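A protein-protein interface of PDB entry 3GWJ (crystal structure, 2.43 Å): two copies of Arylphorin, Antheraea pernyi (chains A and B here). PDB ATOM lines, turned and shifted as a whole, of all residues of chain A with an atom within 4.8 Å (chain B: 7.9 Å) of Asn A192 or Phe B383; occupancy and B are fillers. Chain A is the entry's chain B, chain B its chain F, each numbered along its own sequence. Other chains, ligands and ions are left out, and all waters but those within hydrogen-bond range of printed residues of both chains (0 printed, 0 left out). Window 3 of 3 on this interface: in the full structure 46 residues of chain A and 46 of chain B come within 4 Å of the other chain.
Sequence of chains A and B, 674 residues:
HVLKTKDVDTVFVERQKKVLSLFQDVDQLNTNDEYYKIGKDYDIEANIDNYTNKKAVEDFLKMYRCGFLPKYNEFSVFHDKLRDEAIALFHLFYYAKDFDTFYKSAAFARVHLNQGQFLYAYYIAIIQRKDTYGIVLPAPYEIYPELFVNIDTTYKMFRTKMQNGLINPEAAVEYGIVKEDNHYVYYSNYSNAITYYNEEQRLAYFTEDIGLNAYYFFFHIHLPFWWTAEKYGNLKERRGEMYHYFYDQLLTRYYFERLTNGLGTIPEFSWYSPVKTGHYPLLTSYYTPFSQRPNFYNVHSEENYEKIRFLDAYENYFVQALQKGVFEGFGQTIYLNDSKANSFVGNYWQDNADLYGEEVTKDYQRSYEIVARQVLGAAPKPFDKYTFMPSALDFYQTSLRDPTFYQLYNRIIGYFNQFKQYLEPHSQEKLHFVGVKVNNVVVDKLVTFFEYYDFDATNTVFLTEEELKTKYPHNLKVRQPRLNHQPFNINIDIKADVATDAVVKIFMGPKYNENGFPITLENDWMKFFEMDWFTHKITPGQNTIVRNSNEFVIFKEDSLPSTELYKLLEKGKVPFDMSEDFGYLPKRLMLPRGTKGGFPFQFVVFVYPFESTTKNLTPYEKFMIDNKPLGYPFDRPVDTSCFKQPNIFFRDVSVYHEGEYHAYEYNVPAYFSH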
ATOM      1  N   TYR A 190      -3.155  18.257   6.775  1.00  0.00           N
ATOM      2  CA  TYR A 190      -3.024  17.034   6.004  1.00  0.00           C
ATOM      3  C   TYR A 190      -2.609  17.561   4.625  1.00  0.00           C
ATOM      4  O   TYR A 190      -2.778  18.758   4.350  1.00  0.00           O
ATOM      5  CB  TYR A 190      -4.369  16.309   5.978  1.00  0.00           C
ATOM      6  CG  TYR A 190      -4.774  15.851   7.362  1.00  0.00           C
ATOM      7  CD1 TYR A 190      -3.973  14.959   8.076  1.00  0.00           C
ATOM      8  CD2 TYR A 190      -5.931  16.331   7.976  1.00  0.00           C
ATOM      9  CE1 TYR A 190      -4.311  14.552   9.370  1.00  0.00           C
ATOM     10  CE2 TYR A 190      -6.283  15.932   9.272  1.00  0.00           C
ATOM     11  CZ  TYR A 190      -5.469  15.039   9.963  1.00  0.00           C
ATOM     12  OH  TYR A 190      -5.812  14.606  11.230  1.00  0.00           O
ATOM     13  N   SER A 191      -2.075  16.694   3.766  1.00  0.00           N
ATOM     14  CA  SER A 191      -1.581  17.123   2.447  1.00  0.00           C
ATOM     15  C   SER A 191      -2.567  17.766   1.471  1.00  0.00           C
ATOM     16  O   SER A 191      -2.147  18.485   0.571  1.00  0.00           O
ATOM     17  CB  SER A 191      -0.869  15.965   1.738  1.00  0.00           C
ATOM     18  OG  SER A 191      -1.804  15.008   1.271  1.00  0.00           O
ATOM     19  N   ASN A 192      -3.860  17.526   1.636  1.00  0.00           N
ATOM     20  CA  ASN A 192      -4.840  18.122   0.730  1.00  0.00           C
ATOM     21  C   ASN A 192      -4.934  19.644   0.875  1.00  0.00           C
ATOM     22  O   ASN A 192      -5.554  20.319   0.048  1.00  0.00           O
ATOM     23  CB  ASN A 192      -6.224  17.487   0.935  1.00  0.00           C
ATOM     24  CG  ASN A 192      -6.812  17.779   2.304  1.00  0.00           C
ATOM     25  OD1 ASN A 192      -6.119  17.712   3.317  1.00  0.00           O
ATOM     26  ND2 ASN A 192      -8.104  18.088   2.339  1.00  0.00           N
ATOM     27  N   ALA A 193      -4.307  20.189   1.913  1.00  0.00           N
ATOM     28  CA  ALA A 193      -4.333  21.632   2.130  1.00  0.00           C
ATOM     29  C   ALA A 193      -3.091  22.289   1.537  1.00  0.00           C
ATOM     30  O   ALA A 193      -2.919  23.509   1.619  1.00  0.00           O
ATOM     31  CB  ALA A 193      -4.429  21.940   3.612  1.00  0.00           C
ATOM     32  N   ILE A 194      -2.226  21.482   0.928  1.00  0.00           N
ATOM     33  CA  ILE A 194      -1.009  22.014   0.326  1.00  0.00           C
ATOM     34  C   ILE A 194      -0.843  21.546  -1.133  1.00  0.00           C
ATOM     35  O   ILE A 194      -0.195  22.204  -1.937  1.00  0.00           O
ATOM     36  CB  ILE A 194       0.240  21.611   1.168  1.00  0.00           C
ATOM     37  CG1 ILE A 194       1.450  22.444   0.751  1.00  0.00           C
ATOM     38  CG2 ILE A 194       0.576  20.144   0.965  1.00  0.00           C
ATOM     39  CD1 ILE A 194       1.356  23.908   1.137  1.00  0.00           C
ATOM     40  N   THR A 195      -1.445  20.415  -1.482  1.00  0.00           N
ATOM     41  CA  THR A 195      -1.338  19.896  -2.842  1.00  0.00           C
ATOM     42  C   THR A 195      -2.527  18.990  -3.128  1.00  0.00           C
ATOM     43  O   THR A 195      -2.836  18.088  -2.347  1.00  0.00           O
ATOM     44  CB  THR A 195      -0.013  19.121  -3.029  1.00  0.00           C
ATOM     45  OG1 THR A 195       0.144  18.752  -4.404  1.00  0.00           O
ATOM     46  CG2 THR A 195       0.010  17.875  -2.160  1.00  0.00           C
ATOM     47  N   TYR A 196      -3.206  19.243  -4.243  1.00  0.00           N
ATOM     48  CA  TYR A 196      -4.389  18.468  -4.620  1.00  0.00           C
ATOM     49  C   TYR A 196      -4.192  17.854  -6.009  1.00  0.00           C
ATOM     50  O   TYR A 196      -4.867  18.230  -6.975  1.00  0.00           O
ATOM     51  CB  TYR A 196      -5.601  19.398  -4.604  1.00  0.00           C
ATOM     52  CG  TYR A 196      -6.845  18.787  -4.025  1.00  0.00           C
ATOM     53  CD1 TYR A 196      -7.653  17.940  -4.785  1.00  0.00           C
ATOM     54  CD2 TYR A 196      -7.223  19.056  -2.717  1.00  0.00           C
ATOM     55  CE1 TYR A 196      -8.816  17.380  -4.253  1.00  0.00           C
ATOM     56  CE2 TYR A 196      -8.380  18.501  -2.169  1.00  0.00           C
ATOM     57  CZ  TYR A 196      -9.171  17.669  -2.943  1.00  0.00           C
ATOM     58  OH  TYR A 196     -10.330  17.147  -2.413  1.00  0.00           O
ATOM     59  N   GLN A 201      -7.067  12.982  -2.869  1.00  0.00           N
ATOM     60  CA  GLN A 201      -6.601  13.907  -1.849  1.00  0.00           C
ATOM     61  C   GLN A 201      -7.718  14.328  -0.889  1.00  0.00           C
ATOM     62  O   GLN A 201      -7.455  14.749   0.243  1.00  0.00           O
ATOM     63  CB  GLN A 201      -5.983  15.151  -2.496  1.00  0.00           C
ATOM     64  CG  GLN A 201      -4.513  14.990  -2.907  1.00  0.00           C
ATOM     65  CD  GLN A 201      -3.660  14.415  -1.784  1.00  0.00           C
ATOM     66  OE1 GLN A 201      -3.652  13.197  -1.558  1.00  0.00           O
ATOM     67  NE2 GLN A 201      -2.950  15.287  -1.062  1.00  0.00           N
ATOM     68  N   ALA A 204      -7.516  12.721   2.507  1.00  0.00           N
ATOM     69  CA  ALA A 204      -6.303  12.932   3.306  1.00  0.00           C
ATOM     70  C   ALA A 204      -6.466  12.978   4.817  1.00  0.00           C
ATOM     71  O   ALA A 204      -5.573  12.546   5.527  1.00  0.00           O
ATOM     72  CB  ALA A 204      -5.573  14.191   2.836  1.00  0.00           C
ATOM     73  N   TYR A 664      -8.754  21.281   7.452  1.00  0.00           N
ATOM     74  CA  TYR A 664      -7.811  22.401   7.417  1.00  0.00           C
ATOM     75  C   TYR A 664      -8.361  23.736   7.885  1.00  0.00           C
ATOM     76  O   TYR A 664      -7.601  24.628   8.263  1.00  0.00           O
ATOM     77  CB  TYR A 664      -7.197  22.570   6.025  1.00  0.00           C
ATOM     78  CG  TYR A 664      -8.188  22.713   4.899  1.00  0.00           C
ATOM     79  CD1 TYR A 664      -8.383  21.668   3.990  1.00  0.00           C
ATOM     80  CD2 TYR A 664      -8.920  23.895   4.726  1.00  0.00           C
ATOM     81  CE1 TYR A 664      -9.266  21.795   2.943  1.00  0.00           C
ATOM     82  CE2 TYR A 664      -9.813  24.031   3.676  1.00  0.00           C
ATOM     83  CZ  TYR A 664      -9.978  22.977   2.789  1.00  0.00           C
ATOM     84  OH  TYR A 664     -10.831  23.101   1.727  1.00  0.00           O
ATOM     85  N   PRO B 380       2.648  18.206 -10.271  1.00  0.00           N
ATOM     86  CA  PRO B 380       1.189  18.271 -10.397  1.00  0.00           C
ATOM     87  C   PRO B 380       0.869  19.757 -10.586  1.00  0.00           C
ATOM     88  O   PRO B 380       1.712  20.598 -10.270  1.00  0.00           O
ATOM     89  CB  PRO B 380       0.696  17.758  -9.044  1.00  0.00           C
ATOM     90  CG  PRO B 380       1.813  16.898  -8.555  1.00  0.00           C
ATOM     91  CD  PRO B 380       3.042  17.659  -8.961  1.00  0.00           C
ATOM     92  N   LYS B 381      -0.321  20.097 -11.082  1.00  0.00           N
ATOM     93  CA  LYS B 381      -0.636  21.514 -11.265  1.00  0.00           C
ATOM     94  C   LYS B 381      -0.595  22.217  -9.910  1.00  0.00           C
ATOM     95  O   LYS B 381      -0.873  21.612  -8.871  1.00  0.00           O
ATOM     96  CB  LYS B 381      -2.004  21.716 -11.935  1.00  0.00           C
ATOM     97  CG  LYS B 381      -3.195  21.228 -11.139  1.00  0.00           C
ATOM     98  CD  LYS B 381      -4.498  21.683 -11.787  1.00  0.00           C
ATOM     99  CE  LYS B 381      -4.548  23.203 -11.916  1.00  0.00           C
ATOM    100  NZ  LYS B 381      -5.868  23.676 -12.426  1.00  0.00           N
ATOM    101  N   PRO B 382      -0.234  23.505  -9.909  1.00  0.00           N
ATOM    102  CA  PRO B 382      -0.144  24.293  -8.680  1.00  0.00           C
ATOM    103  C   PRO B 382      -1.407  24.272  -7.863  1.00  0.00           C
ATOM    104  O   PRO B 382      -2.505  24.254  -8.410  1.00  0.00           O
ATOM    105  CB  PRO B 382       0.194  25.689  -9.189  1.00  0.00           C
ATOM    106  CG  PRO B 382       1.018  25.381 -10.427  1.00  0.00           C
ATOM    107  CD  PRO B 382       0.178  24.309 -11.072  1.00  0.00           C
ATOM    108  N   PHE B 383      -1.229  24.254  -6.545  1.00  0.00           N
ATOM    109  CA  PHE B 383      -2.339  24.257  -5.606  1.00  0.00           C
ATOM    110  C   PHE B 383      -3.112  25.560  -5.820  1.00  0.00           C
ATOM    111  O   PHE B 383      -4.331  25.559  -5.901  1.00  0.00           O
ATOM    112  CB  PHE B 383      -1.797  24.167  -4.181  1.00  0.00           C
ATOM    113  CG  PHE B 383      -2.855  24.193  -3.133  1.00  0.00           C
ATOM    114  CD1 PHE B 383      -3.002  25.305  -2.307  1.00  0.00           C
ATOM    115  CD2 PHE B 383      -3.711  23.107  -2.968  1.00  0.00           C
ATOM    116  CE1 PHE B 383      -3.986  25.337  -1.326  1.00  0.00           C
ATOM    117  CE2 PHE B 383      -4.697  23.128  -1.994  1.00  0.00           C
ATOM    118  CZ  PHE B 383      -4.836  24.249  -1.168  1.00  0.00           C
ATOM    119  N   ASP B 384      -2.378  26.669  -5.904  1.00  0.00           N
ATOM    120  CA  ASP B 384      -2.957  27.984  -6.162  1.00  0.00           C
ATOM    121  C   ASP B 384      -1.821  28.904  -6.643  1.00  0.00           C
ATOM    122  O   ASP B 384      -0.673  28.470  -6.727  1.00  0.00           O
ATOM    123  CB  ASP B 384      -3.689  28.534  -4.919  1.00  0.00           C
ATOM    124  CG  ASP B 384      -2.754  28.881  -3.765  1.00  0.00           C
ATOM    125  OD1 ASP B 384      -3.224  28.857  -2.606  1.00  0.00           O
ATOM    126  OD2 ASP B 384      -1.572  29.201  -4.000  1.00  0.00           O
ATOM    127  N   LYS B 385      -2.128  30.155  -6.969  1.00  0.00           N
ATOM    128  CA  LYS B 385      -1.103  31.059  -7.490  1.00  0.00           C
ATOM    129  C   LYS B 385       0.163  31.212  -6.650  1.00  0.00           C
ATOM    130  O   LYS B 385       1.229  31.523  -7.173  1.00  0.00           O
ATOM    131  CB  LYS B 385      -1.697  32.442  -7.741  1.00  0.00           C
ATOM    132  CG  LYS B 385      -2.178  33.152  -6.492  1.00  0.00           C
ATOM    133  CD  LYS B 385      -2.522  34.594  -6.797  1.00  0.00           C
ATOM    134  CE  LYS B 385      -2.895  35.345  -5.529  1.00  0.00           C
ATOM    135  NZ  LYS B 385      -2.940  36.810  -5.787  1.00  0.00           N
ATOM    136  N   TYR B 386       0.056  30.977  -5.353  1.00  0.00           N
ATOM    137  CA  TYR B 386       1.203  31.136  -4.479  1.00  0.00           C
ATOM    138  C   TYR B 386       1.833  29.830  -4.010  1.00  0.00           C
ATOM    139  O   TYR B 386       2.875  29.849  -3.359  1.00  0.00           O
ATOM    140  CB  TYR B 386       0.777  31.949  -3.262  1.00  0.00           C
ATOM    141  CG  TYR B 386       0.597  33.430  -3.517  1.00  0.00           C
ATOM    142  CD1 TYR B 386      -0.295  34.186  -2.749  1.00  0.00           C
ATOM    143  CD2 TYR B 386       1.366  34.092  -4.475  1.00  0.00           C
ATOM    144  CE1 TYR B 386      -0.415  35.560  -2.923  1.00  0.00           C
ATOM    145  CE2 TYR B 386       1.258  35.472  -4.658  1.00  0.00           C
ATOM    146  CZ  TYR B 386       0.368  36.198  -3.878  1.00  0.00           C
ATOM    147  OH  TYR B 386       0.288  37.563  -4.038  1.00  0.00           O
ATOM    148  N   THR B 387       1.214  28.703  -4.352  1.00  0.00           N
ATOM    149  CA  THR B 387       1.692  27.405  -3.900  1.00  0.00           C
ATOM    150  C   THR B 387       1.846  26.365  -5.000  1.00  0.00           C
ATOM    151  O   THR B 387       0.872  25.989  -5.648  1.00  0.00           O
ATOM    152  CB  THR B 387       0.734  26.849  -2.842  1.00  0.00           C
ATOM    153  OG1 THR B 387       0.542  27.833  -1.817  1.00  0.00           O
ATOM    154  CG2 THR B 387       1.277  25.560  -2.237  1.00  0.00           C
ATOM    155  N   PHE B 388       3.069  25.885  -5.190  1.00  0.00           N
ATOM    156  CA  PHE B 388       3.343  24.879  -6.210  1.00  0.00           C
ATOM    157  C   PHE B 388       4.451  23.935  -5.763  1.00  0.00           C
ATOM    158  O   PHE B 388       5.248  24.266  -4.893  1.00  0.00           O
ATOM    159  CB  PHE B 388       3.761  25.544  -7.523  1.00  0.00           C
ATOM    160  CG  PHE B 388       5.043  26.313  -7.429  1.00  0.00           C
ATOM    161  CD1 PHE B 388       5.056  27.621  -6.958  1.00  0.00           C
ATOM    162  CD2 PHE B 388       6.252  25.716  -7.767  1.00  0.00           C
ATOM    163  CE1 PHE B 388       6.253  28.317  -6.825  1.00  0.00           C
ATOM    164  CE2 PHE B 388       7.452  26.408  -7.636  1.00  0.00           C
ATOM    165  CZ  PHE B 388       7.450  27.709  -7.163  1.00  0.00           C
ATOM    166  N   MET B 389       4.492  22.751  -6.358  1.00  0.00           N
ATOM    167  CA  MET B 389       5.531  21.778  -6.033  1.00  0.00           C
ATOM    168  C   MET B 389       6.602  22.042  -7.084  1.00  0.00           C
ATOM    169  O   MET B 389       6.399  21.792  -8.271  1.00  0.00           O
ATOM    170  CB  MET B 389       4.993  20.344  -6.151  1.00  0.00           C
ATOM    171  CG  MET B 389       6.004  19.278  -5.790  1.00  0.00           C
ATOM    172  SD  MET B 389       5.367  17.605  -6.010  1.00  0.00           S
ATOM    173  CE  MET B 389       3.994  17.619  -4.768  1.00  0.00           C
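No position is printed for both chains. Of the 5 pairs that touch across the chains among the printed residues, none has its exchanged pair printed and touching as well.
The side-chain amide nitrogen of Gln A201 is in hydrogen-bond range of the backbone carbonyl oxygen of Thr A195 (3.1 Å). The side-chain carboxylate of Asp B384 sits at hydrogen-bond distance from the backbone NH of Thr B387 (2.9 Å).
Printed residues of chain B that touch a printed residue of chain A: Phe B383 and Thr B387. Hydrophobic or aromatic side chains of chain B that line the printed part of chain A: Phe B383. Printed residues of chain A that touch a printed residue of chain B: Asn A192, Ala A193, Ile A194 and Thr A195. Along chain A the printed residues that touch a printed residue of chain B span positions 192 to 195. Among the printed residues, 5 pairs touch across the chains.
Of chain B, only Phe B383 comes within 4 Å of Asn A192. Of chain B, only Phe B383 (3.5 Å) comes within 4 Å of Ala A193. Of the printed residues of chain B, Ile A194 touches Phe B383 and Thr B387. Of the printed residues of chain B, Thr A195 touches Phe B383. Lys B381 touches none of the printed residues of chain A. Phe B383 touches just these residues of chain A: Asn A192, Ala A193, Ile A194 and Thr A195. Of the printed residues of chain A, Thr B387 touches Ile A194 (3.7 Å). Met B389 touches none of the printed residues of chain A. The nearest residue of chain A that does not touch Phe B383 is Tyr A196 (4.1 Å).
Asn A192 touches Phe B383 (O to CE2, 3.6 Å). Phe B383 touches Ala A193 (CZ to O, 3.5 Å). Phe B383 touches Ile A194. Ile A194 touches Thr B387. N of Thr A195 touches CD2 of Phe B383, 3.8 Å away.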
